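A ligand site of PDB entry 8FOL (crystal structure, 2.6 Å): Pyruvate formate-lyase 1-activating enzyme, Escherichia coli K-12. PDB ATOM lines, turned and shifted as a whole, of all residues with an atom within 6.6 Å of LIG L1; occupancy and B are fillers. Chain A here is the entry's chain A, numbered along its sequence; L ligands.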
ATOM      1  N   GLY A  28     -31.767  18.385 -20.965  1.00  0.00           N
ATOM      2  CA  GLY A  28     -30.657  18.263 -21.907  1.00  0.00           C
ATOM      3  C   GLY A  28     -29.286  18.247 -21.257  1.00  0.00           C
ATOM      4  O   GLY A  28     -28.944  19.156 -20.495  1.00  0.00           O
ATOM      5  N   CYS A  29     -28.508  17.215 -21.540  1.00  0.00           N
ATOM      6  CA  CYS A  29     -27.136  17.120 -21.059  1.00  0.00           C
ATOM      7  C   CYS A  29     -26.309  16.317 -22.056  1.00  0.00           C
ATOM      8  O   CYS A  29     -26.819  15.375 -22.674  1.00  0.00           O
ATOM      9  CB  CYS A  29     -27.067  16.469 -19.675  1.00  0.00           C
ATOM     10  SG  CYS A  29     -25.393  16.351 -18.991  1.00  0.00           S
ATOM     11  N   LEU A  30     -25.047  16.687 -22.208  1.00  0.00           N
ATOM     12  CA  LEU A  30     -24.139  16.022 -23.136  1.00  0.00           C
ATOM     13  C   LEU A  30     -23.060  15.194 -22.446  1.00  0.00           C
ATOM     14  O   LEU A  30     -22.167  14.685 -23.130  1.00  0.00           O
ATOM     15  CB  LEU A  30     -23.497  17.043 -24.080  1.00  0.00           C
ATOM     16  CG  LEU A  30     -24.516  17.887 -24.841  1.00  0.00           C
ATOM     17  CD1 LEU A  30     -23.816  18.927 -25.693  1.00  0.00           C
ATOM     18  CD2 LEU A  30     -25.412  16.996 -25.686  1.00  0.00           C
ATOM     19  N   MET A  31     -23.108  15.054 -21.126  1.00  0.00           N
ATOM     20  CA  MET A  31     -22.265  14.099 -20.426  1.00  0.00           C
ATOM     21  C   MET A  31     -23.038  12.830 -20.125  1.00  0.00           C
ATOM     22  O   MET A  31     -24.280  12.797 -20.189  1.00  0.00           O
ATOM     23  CB  MET A  31     -21.722  14.696 -19.123  1.00  0.00           C
ATOM     24  CG  MET A  31     -20.564  15.665 -19.316  1.00  0.00           C
ATOM     25  SD  MET A  31     -19.914  16.258 -17.739  1.00  0.00           S
ATOM     26  CE  MET A  31     -18.407  17.045 -18.309  1.00  0.00           C
ATOM     27  N   ARG A  32     -22.310  11.771 -19.788  1.00  0.00           N
ATOM     28  CA  ARG A  32     -22.886  10.433 -19.626  1.00  0.00           C
ATOM     29  C   ARG A  32     -22.386   9.783 -18.341  1.00  0.00           C
ATOM     30  O   ARG A  32     -21.918   8.641 -18.339  1.00  0.00           O
ATOM     31  CB  ARG A  32     -22.554   9.570 -20.839  1.00  0.00           C
ATOM     32  CG  ARG A  32     -23.056  10.133 -22.175  1.00  0.00           C
ATOM     33  CD  ARG A  32     -24.578  10.177 -22.211  1.00  0.00           C
ATOM     34  NE  ARG A  32     -25.128  10.662 -23.465  1.00  0.00           N
ATOM     35  CZ  ARG A  32     -25.643  11.873 -23.656  1.00  0.00           C
ATOM     36  NH1 ARG A  32     -25.676  12.743 -22.654  1.00  0.00           N
ATOM     37  NH2 ARG A  32     -26.129  12.220 -24.828  1.00  0.00           N
ATOM     38  N   CYS A  33     -22.513  10.494 -17.216  1.00  0.00           N
ATOM     39  CA  CYS A  33     -22.018   9.984 -15.944  1.00  0.00           C
ATOM     40  C   CYS A  33     -22.732   8.687 -15.587  1.00  0.00           C
ATOM     41  O   CYS A  33     -23.963   8.610 -15.585  1.00  0.00           O
ATOM     42  CB  CYS A  33     -22.231  11.002 -14.833  1.00  0.00           C
ATOM     43  SG  CYS A  33     -21.677  12.670 -15.207  1.00  0.00           S
ATOM     44  N   LEU A  34     -21.933   7.659 -15.272  1.00  0.00           N
ATOM     45  CA  LEU A  34     -22.490   6.358 -14.892  1.00  0.00           C
ATOM     46  C   LEU A  34     -23.403   6.463 -13.682  1.00  0.00           C
ATOM     47  O   LEU A  34     -24.276   5.600 -13.501  1.00  0.00           O
ATOM     48  CB  LEU A  34     -21.362   5.368 -14.608  1.00  0.00           C
ATOM     49  CG  LEU A  34     -20.158   5.345 -15.567  1.00  0.00           C
ATOM     50  CD1 LEU A  34     -19.218   4.199 -15.190  1.00  0.00           C
ATOM     51  CD2 LEU A  34     -20.596   5.232 -17.017  1.00  0.00           C
ATOM     52  N   TYR A  35     -23.241   7.495 -12.846  1.00  0.00           N
ATOM     53  CA  TYR A  35     -23.974   7.590 -11.592  1.00  0.00           C
ATOM     54  C   TYR A  35     -25.135   8.570 -11.651  1.00  0.00           C
ATOM     55  O   TYR A  35     -25.735   8.854 -10.610  1.00  0.00           O
ATOM     56  CB  TYR A  35     -23.016   7.976 -10.444  1.00  0.00           C
ATOM     57  CG  TYR A  35     -22.209   9.241 -10.655  1.00  0.00           C
ATOM     58  CD1 TYR A  35     -22.812  10.497 -10.618  1.00  0.00           C
ATOM     59  CD2 TYR A  35     -20.829   9.192 -10.844  1.00  0.00           C
ATOM     60  CE1 TYR A  35     -22.078  11.649 -10.792  1.00  0.00           C
ATOM     61  CE2 TYR A  35     -20.087  10.354 -11.025  1.00  0.00           C
ATOM     62  CZ  TYR A  35     -20.725  11.582 -10.994  1.00  0.00           C
ATOM     63  OH  TYR A  35     -20.012  12.742 -11.166  1.00  0.00           O
ATOM     64  N   CYS A  36     -25.492   9.067 -12.833  1.00  0.00           N
ATOM     65  CA  CYS A  36     -26.486  10.129 -12.968  1.00  0.00           C
ATOM     66  C   CYS A  36     -27.808   9.736 -12.320  1.00  0.00           C
ATOM     67  O   CYS A  36     -28.431   8.748 -12.707  1.00  0.00           O
ATOM     68  CB  CYS A  36     -26.710  10.465 -14.432  1.00  0.00           C
ATOM     69  SG  CYS A  36     -27.806  11.872 -14.703  1.00  0.00           S
ATOM     70  N   HIS A  37     -28.243  10.524 -11.343  1.00  0.00           N
ATOM     71  CA  HIS A  37     -29.531  10.277 -10.713  1.00  0.00           C
ATOM     72  C   HIS A  37     -30.678  10.982 -11.420  1.00  0.00           C
ATOM     73  O   HIS A  37     -31.835  10.847 -11.009  1.00  0.00           O
ATOM     74  CB  HIS A  37     -29.492  10.681  -9.226  1.00  0.00           C
ATOM     75  CG  HIS A  37     -29.209  12.134  -8.969  1.00  0.00           C
ATOM     76  ND1 HIS A  37     -28.706  12.583  -7.760  1.00  0.00           N
ATOM     77  CD2 HIS A  37     -29.364  13.233  -9.746  1.00  0.00           C
ATOM     78  CE1 HIS A  37     -28.565  13.897  -7.815  1.00  0.00           C
ATOM     79  NE2 HIS A  37     -28.964  14.311  -9.000  1.00  0.00           N
ATOM     80  N   ASN A  38     -30.386  11.736 -12.490  1.00  0.00           N
ATOM     81  CA  ASN A  38     -31.422  12.367 -13.308  1.00  0.00           C
ATOM     82  C   ASN A  38     -31.274  11.919 -14.752  1.00  0.00           C
ATOM     83  O   ASN A  38     -31.151  12.746 -15.659  1.00  0.00           O
ATOM     84  CB  ASN A  38     -31.336  13.898 -13.206  1.00  0.00           C
ATOM     85  CG  ASN A  38     -31.655  14.411 -11.820  1.00  0.00           C
ATOM     86  OD1 ASN A  38     -32.394  13.779 -11.062  1.00  0.00           O
ATOM     87  ND2 ASN A  38     -31.105  15.565 -11.484  1.00  0.00           N
ATOM     88  N   ARG A  39     -31.293  10.599 -14.961  1.00  0.00           N
ATOM     89  CA  ARG A  39     -31.032  10.040 -16.289  1.00  0.00           C
ATOM     90  C   ARG A  39     -32.014  10.562 -17.332  1.00  0.00           C
ATOM     91  O   ARG A  39     -31.646  10.720 -18.504  1.00  0.00           O
ATOM     92  CB  ARG A  39     -31.075   8.514 -16.219  1.00  0.00           C
ATOM     93  CG  ARG A  39     -31.074   7.797 -17.550  1.00  0.00           C
ATOM     94  CD  ARG A  39     -29.845   8.122 -18.385  1.00  0.00           C
ATOM     95  NE  ARG A  39     -29.904   7.468 -19.693  1.00  0.00           N
ATOM     96  CZ  ARG A  39     -30.545   7.951 -20.746  1.00  0.00           C
ATOM     97  NH1 ARG A  39     -31.196   9.111 -20.650  1.00  0.00           N
ATOM     98  NH2 ARG A  39     -30.551   7.289 -21.891  1.00  0.00           N
ATOM     99  N   THR A  41     -32.971  13.446 -17.897  1.00  0.00           N
ATOM    100  CA  THR A  41     -32.703  14.825 -18.285  1.00  0.00           C
ATOM    101  C   THR A  41     -31.691  14.926 -19.415  1.00  0.00           C
ATOM    102  O   THR A  41     -31.288  16.032 -19.778  1.00  0.00           O
ATOM    103  CB  THR A  41     -32.220  15.650 -17.077  1.00  0.00           C
ATOM    104  OG1 THR A  41     -30.940  15.182 -16.643  1.00  0.00           O
ATOM    105  CG2 THR A  41     -33.212  15.558 -15.927  1.00  0.00           C
ATOM    106  N   TRP A  42     -31.261  13.804 -19.995  1.00  0.00           N
ATOM    107  CA  TRP A  42     -30.219  13.818 -21.010  1.00  0.00           C
ATOM    108  C   TRP A  42     -30.731  14.332 -22.354  1.00  0.00           C
ATOM    109  O   TRP A  42     -30.088  15.172 -22.985  1.00  0.00           O
ATOM    110  CB  TRP A  42     -29.620  12.423 -21.190  1.00  0.00           C
ATOM    111  CG  TRP A  42     -28.808  11.977 -20.039  1.00  0.00           C
ATOM    112  CD1 TRP A  42     -28.637  12.625 -18.847  1.00  0.00           C
ATOM    113  CD2 TRP A  42     -28.030  10.776 -19.964  1.00  0.00           C
ATOM    114  NE1 TRP A  42     -27.793  11.896 -18.031  1.00  0.00           N
ATOM    115  CE2 TRP A  42     -27.409  10.759 -18.697  1.00  0.00           C
ATOM    116  CE3 TRP A  42     -27.792   9.723 -20.850  1.00  0.00           C
ATOM    117  CZ2 TRP A  42     -26.576   9.728 -18.292  1.00  0.00           C
ATOM    118  CZ3 TRP A  42     -26.967   8.696 -20.447  1.00  0.00           C
ATOM    119  CH2 TRP A  42     -26.367   8.709 -19.176  1.00  0.00           C
ATOM    120  N   GLY A  77     -30.383  20.676 -13.567  1.00  0.00           N
ATOM    121  CA  GLY A  77     -30.824  19.766 -14.600  1.00  0.00           C
ATOM    122  C   GLY A  77     -30.281  18.361 -14.435  1.00  0.00           C
ATOM    123  O   GLY A  77     -30.355  17.797 -13.333  1.00  0.00           O
ATOM    124  N   GLY A  78     -29.734  17.779 -15.489  1.00  0.00           N
ATOM    125  CA  GLY A  78     -29.560  18.455 -16.758  1.00  0.00           C
ATOM    126  C   GLY A  78     -28.394  19.422 -16.696  1.00  0.00           C
ATOM    127  O   GLY A  78     -27.819  19.645 -15.638  1.00  0.00           O
ATOM    128  N   GLU A  79     -28.039  20.013 -17.840  1.00  0.00           N
ATOM    129  CA  GLU A  79     -26.973  20.997 -17.896  1.00  0.00           C
ATOM    130  C   GLU A  79     -27.562  22.328 -18.349  1.00  0.00           C
ATOM    131  O   GLU A  79     -27.850  22.518 -19.536  1.00  0.00           O
ATOM    132  CB  GLU A  79     -25.845  20.537 -18.813  1.00  0.00           C
ATOM    133  CG  GLU A  79     -24.674  21.494 -18.806  1.00  0.00           C
ATOM    134  CD  GLU A  79     -24.356  22.019 -17.419  1.00  0.00           C
ATOM    135  OE1 GLU A  79     -24.189  21.198 -16.485  1.00  0.00           O
ATOM    136  OE2 GLU A  79     -24.298  23.253 -17.243  1.00  0.00           O
ATOM    137  N   ASN A 106     -21.953  21.452 -14.911  1.00  0.00           N
ATOM    138  CA  ASN A 106     -20.800  20.589 -15.075  1.00  0.00           C
ATOM    139  C   ASN A 106     -19.654  21.259 -15.820  1.00  0.00           C
ATOM    140  O   ASN A 106     -18.610  20.633 -16.033  1.00  0.00           O
ATOM    141  CB  ASN A 106     -21.191  19.290 -15.801  1.00  0.00           C
ATOM    142  CG  ASN A 106     -21.766  19.540 -17.182  1.00  0.00           C
ATOM    143  OD1 ASN A 106     -21.573  20.593 -17.781  1.00  0.00           O
ATOM    144  ND2 ASN A 106     -22.493  18.551 -17.701  1.00  0.00           N
ATOM    145  N   ASP A 129     -19.096  21.165 -10.890  1.00  0.00           N
ATOM    146  CA  ASP A 129     -18.765  19.757 -10.674  1.00  0.00           C
ATOM    147  C   ASP A 129     -17.438  19.438 -11.331  1.00  0.00           C
ATOM    148  O   ASP A 129     -17.317  19.514 -12.560  1.00  0.00           O
ATOM    149  CB  ASP A 129     -19.864  18.854 -11.224  1.00  0.00           C
ATOM    150  CG  ASP A 129     -20.722  18.264 -10.132  1.00  0.00           C
ATOM    151  OD1 ASP A 129     -21.298  19.050  -9.347  1.00  0.00           O
ATOM    152  OD2 ASP A 129     -20.816  17.013 -10.052  1.00  0.00           O
ATOM    153  N   LYS A 131     -15.688  16.217 -11.697  1.00  0.00           N
ATOM    154  CA  LYS A 131     -16.053  14.830 -11.471  1.00  0.00           C
ATOM    155  C   LYS A 131     -14.840  13.914 -11.308  1.00  0.00           C
ATOM    156  O   LYS A 131     -14.922  12.916 -10.582  1.00  0.00           O
ATOM    157  CB  LYS A 131     -16.949  14.339 -12.611  1.00  0.00           C
ATOM    158  CG  LYS A 131     -18.283  15.072 -12.644  1.00  0.00           C
ATOM    159  CD  LYS A 131     -19.063  14.785 -13.904  1.00  0.00           C
ATOM    160  CE  LYS A 131     -20.295  15.678 -13.989  1.00  0.00           C
ATOM    161  NZ  LYS A 131     -21.294  15.328 -12.950  1.00  0.00           N
ATOM    162  N   VAL A 142     -17.484   9.448 -17.245  1.00  0.00           N
ATOM    163  CA  VAL A 142     -18.388  10.461 -17.769  1.00  0.00           C
ATOM    164  C   VAL A 142     -18.642  10.304 -19.263  1.00  0.00           C
ATOM    165  O   VAL A 142     -19.690  10.767 -19.751  1.00  0.00           O
ATOM    166  CB  VAL A 142     -17.854  11.877 -17.474  1.00  0.00           C
ATOM    167  CG1 VAL A 142     -18.906  12.915 -17.766  1.00  0.00           C
ATOM    168  CG2 VAL A 142     -17.411  11.977 -16.024  1.00  0.00           C
HETATM  169 FE1  LIG L   1     -23.603  13.856 -15.348  1.00  0.00          FE
HETATM  170 FE2  LIG L   1     -25.157  15.859 -14.285  1.00  0.00          FE
HETATM  171 FE3  LIG L   1     -26.312  13.519 -15.135  1.00  0.00          FE
HETATM  172 FE4  LIG L   1     -25.281  15.295 -16.966  1.00  0.00          FE
HETATM  173  S1  LIG L   1     -27.048  15.641 -15.567  1.00  0.00           S
HETATM  174  S2  LIG L   1     -25.003  13.022 -16.937  1.00  0.00           S
HETATM  175  S3  LIG L   1     -23.482  16.087 -15.820  1.00  0.00           S
HETATM  176  S4  LIG L   1     -24.829  13.775 -13.425  1.00  0.00           S
HETATM  177  N1  LG2 L   2     -25.656  18.415 -14.625  1.00  0.00           N
HETATM  178  C1  LG2 L   2     -25.036  19.230 -13.599  1.00  0.00           C
HETATM  179  C2  LG2 L   2     -23.863  18.468 -12.973  1.00  0.00           C
HETATM  180  O1  LG2 L   2     -23.888  17.211 -12.896  1.00  0.00           O
HETATM  181  O2  LG2 L   2     -22.873  19.100 -12.534  1.00  0.00           O
HETATM  182  C3  LG2 L   2     -26.062  19.616 -12.524  1.00  0.00           C
HETATM  183  C4  LG2 L   2     -27.169  18.569 -12.414  1.00  0.00           C
HETATM  184  S1  LG2 L   2     -26.724  17.301 -11.320  1.00  0.00           S
HETATM  185  C5  LG2 L   2     -27.701  15.909 -11.639  1.00  0.00           C
HETATM  186  C6  LG2 L   2     -26.901  17.827  -9.697  1.00  0.00           C
HETATM  187  C7  LG2 L   2     -25.831  17.227  -8.710  1.00  0.00           C
HETATM  188  O3  LG2 L   2     -26.152  15.836  -8.323  1.00  0.00           O
HETATM  189  C8  LG2 L   2     -24.404  17.195  -9.303  1.00  0.00           C
HETATM  190  O4  LG2 L   2     -23.447  17.622  -8.315  1.00  0.00           O
HETATM  191  C9  LG2 L   2     -24.217  15.715  -9.611  1.00  0.00           C
HETATM  192  O5  LG2 L   2     -22.814  15.367  -9.672  1.00  0.00           O
HETATM  193  C10 LG2 L   2     -24.896  15.092  -8.380  1.00  0.00           C
HETATM  194  N2  LG2 L   2     -25.164  13.686  -8.582  1.00  0.00           N
HETATM  195  C11 LG2 L   2     -25.615  13.104  -9.703  1.00  0.00           C
HETATM  196  N3  LG2 L   2     -25.724  11.784  -9.460  1.00  0.00           N
HETATM  197  C12 LG2 L   2     -25.340  11.557  -8.202  1.00  0.00           C
HETATM  198  C13 LG2 L   2     -25.256  10.394  -7.451  1.00  0.00           C
HETATM  199  N4  LG2 L   2     -25.637   9.123  -8.040  1.00  0.00           N
HETATM  200  N5  LG2 L   2     -24.826  10.452  -6.205  1.00  0.00           N
HETATM  201  C14 LG2 L   2     -24.475  11.634  -5.658  1.00  0.00           C
HETATM  202  N6  LG2 L   2     -24.557  12.770  -6.389  1.00  0.00           N
HETATM  203  C15 LG2 L   2     -24.992  12.731  -7.657  1.00  0.00           C
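NE1 of Trp 42 sits close to SG of Cys 36. SG of Cys 36 lies close to N of Asn 38 (3.4 Å). The side-chain sulfur (SG) of Cys 36 sits close to the backbone NH (N) of Arg 39 (3.7 Å). SG of Cys 29 lies close to N of Met 31, at 3.4 Å. The backbone NH (N) of Cys 29 lies within hydrogen-bond range of the backbone carbonyl oxygen (O) of Thr 41 (3.5 Å). The side-chain amide nitrogen of Asn 106 is in hydrogen-bond range of the side-chain sulfur of Met 31, 3.5 Å away. The backbone NH of Gly 78 is in hydrogen-bond range of the side-chain hydroxyl of Thr 41, 3.1 Å away. OD2 of Asp 129 is in salt-bridge range of NZ of Lys 131 (3.4 Å).
An iron atom (FE2) of LIG L1 is bound by an oxygen (O1) of LG2 L2, at 2.3 Å.
FE3 of LIG L1 is bound by SG of Cys 36, at 2.3 Å. The backbone NH (N) of Cys 33 sits close to a sulfur (S2) of LIG L1 (3.6 Å). FE1 of LIG L1 is bound by SG of Cys 33, at 2.3 Å. The side-chain sulfur of Cys 29 binds an iron atom (FE4) of LIG L1. The indole nitrogen of Trp 42 lies close to a sulfur (S2) of LIG L1, at 3.2 Å. The side-chain amide nitrogen of Asn 106 sits close to a sulfur (S3) of LIG L1 (3.3 Å). The backbone NH (N) of Gly 78 sits close to a sulfur (S1) of LIG L1 (3.4 Å). A sulfur (S3) of LIG L1 sits close to the side-chain amino group of Lys 131 (3.7 Å). The backbone NH (N) of Asn 106 is in hydrogen-bond range of an oxygen (O2) of LG2 L2 (3.5 Å). The backbone carbonyl oxygen (O) of Gly 78 sits at hydrogen-bond distance from a nitrogen (N1) of LG2 L2 (2.7 Å). The side-chain amino group of Lys 131 sits close to an oxygen (O1) of LG2 L2, at 3.2 Å. The backbone carbonyl oxygen of Tyr 35 lies within hydrogen-bond range of a nitrogen (N4) of LG2 L2 (2.6 Å). OE1 of Glu 79 lies within salt-bridge range of N1 of LG2 L2, at 3.7 Å. N of His 37 lies within hydrogen-bond range of N3 of LG2 L2. An oxygen (O3) of LG2 L2 lies close to a ring nitrogen (NE2) of His 37 (3.3 Å). OD2 of Asp 129 is in hydrogen-bond range of O5 of LG2 L2 (2.6 Å).
The backbone carbonyl oxygen (O) of Met 31 lies close to a sulfur (S2) of LIG L1, 3.3 Å away. Of the 21 residues printed, 8 come within 4 Å of LIG L1. Along chain A the residues within 4 Å of LIG L1 span positions 29 to 131. The nearest printed residue that does not touch LIG L1 is Thr 41 (4.1 Å).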
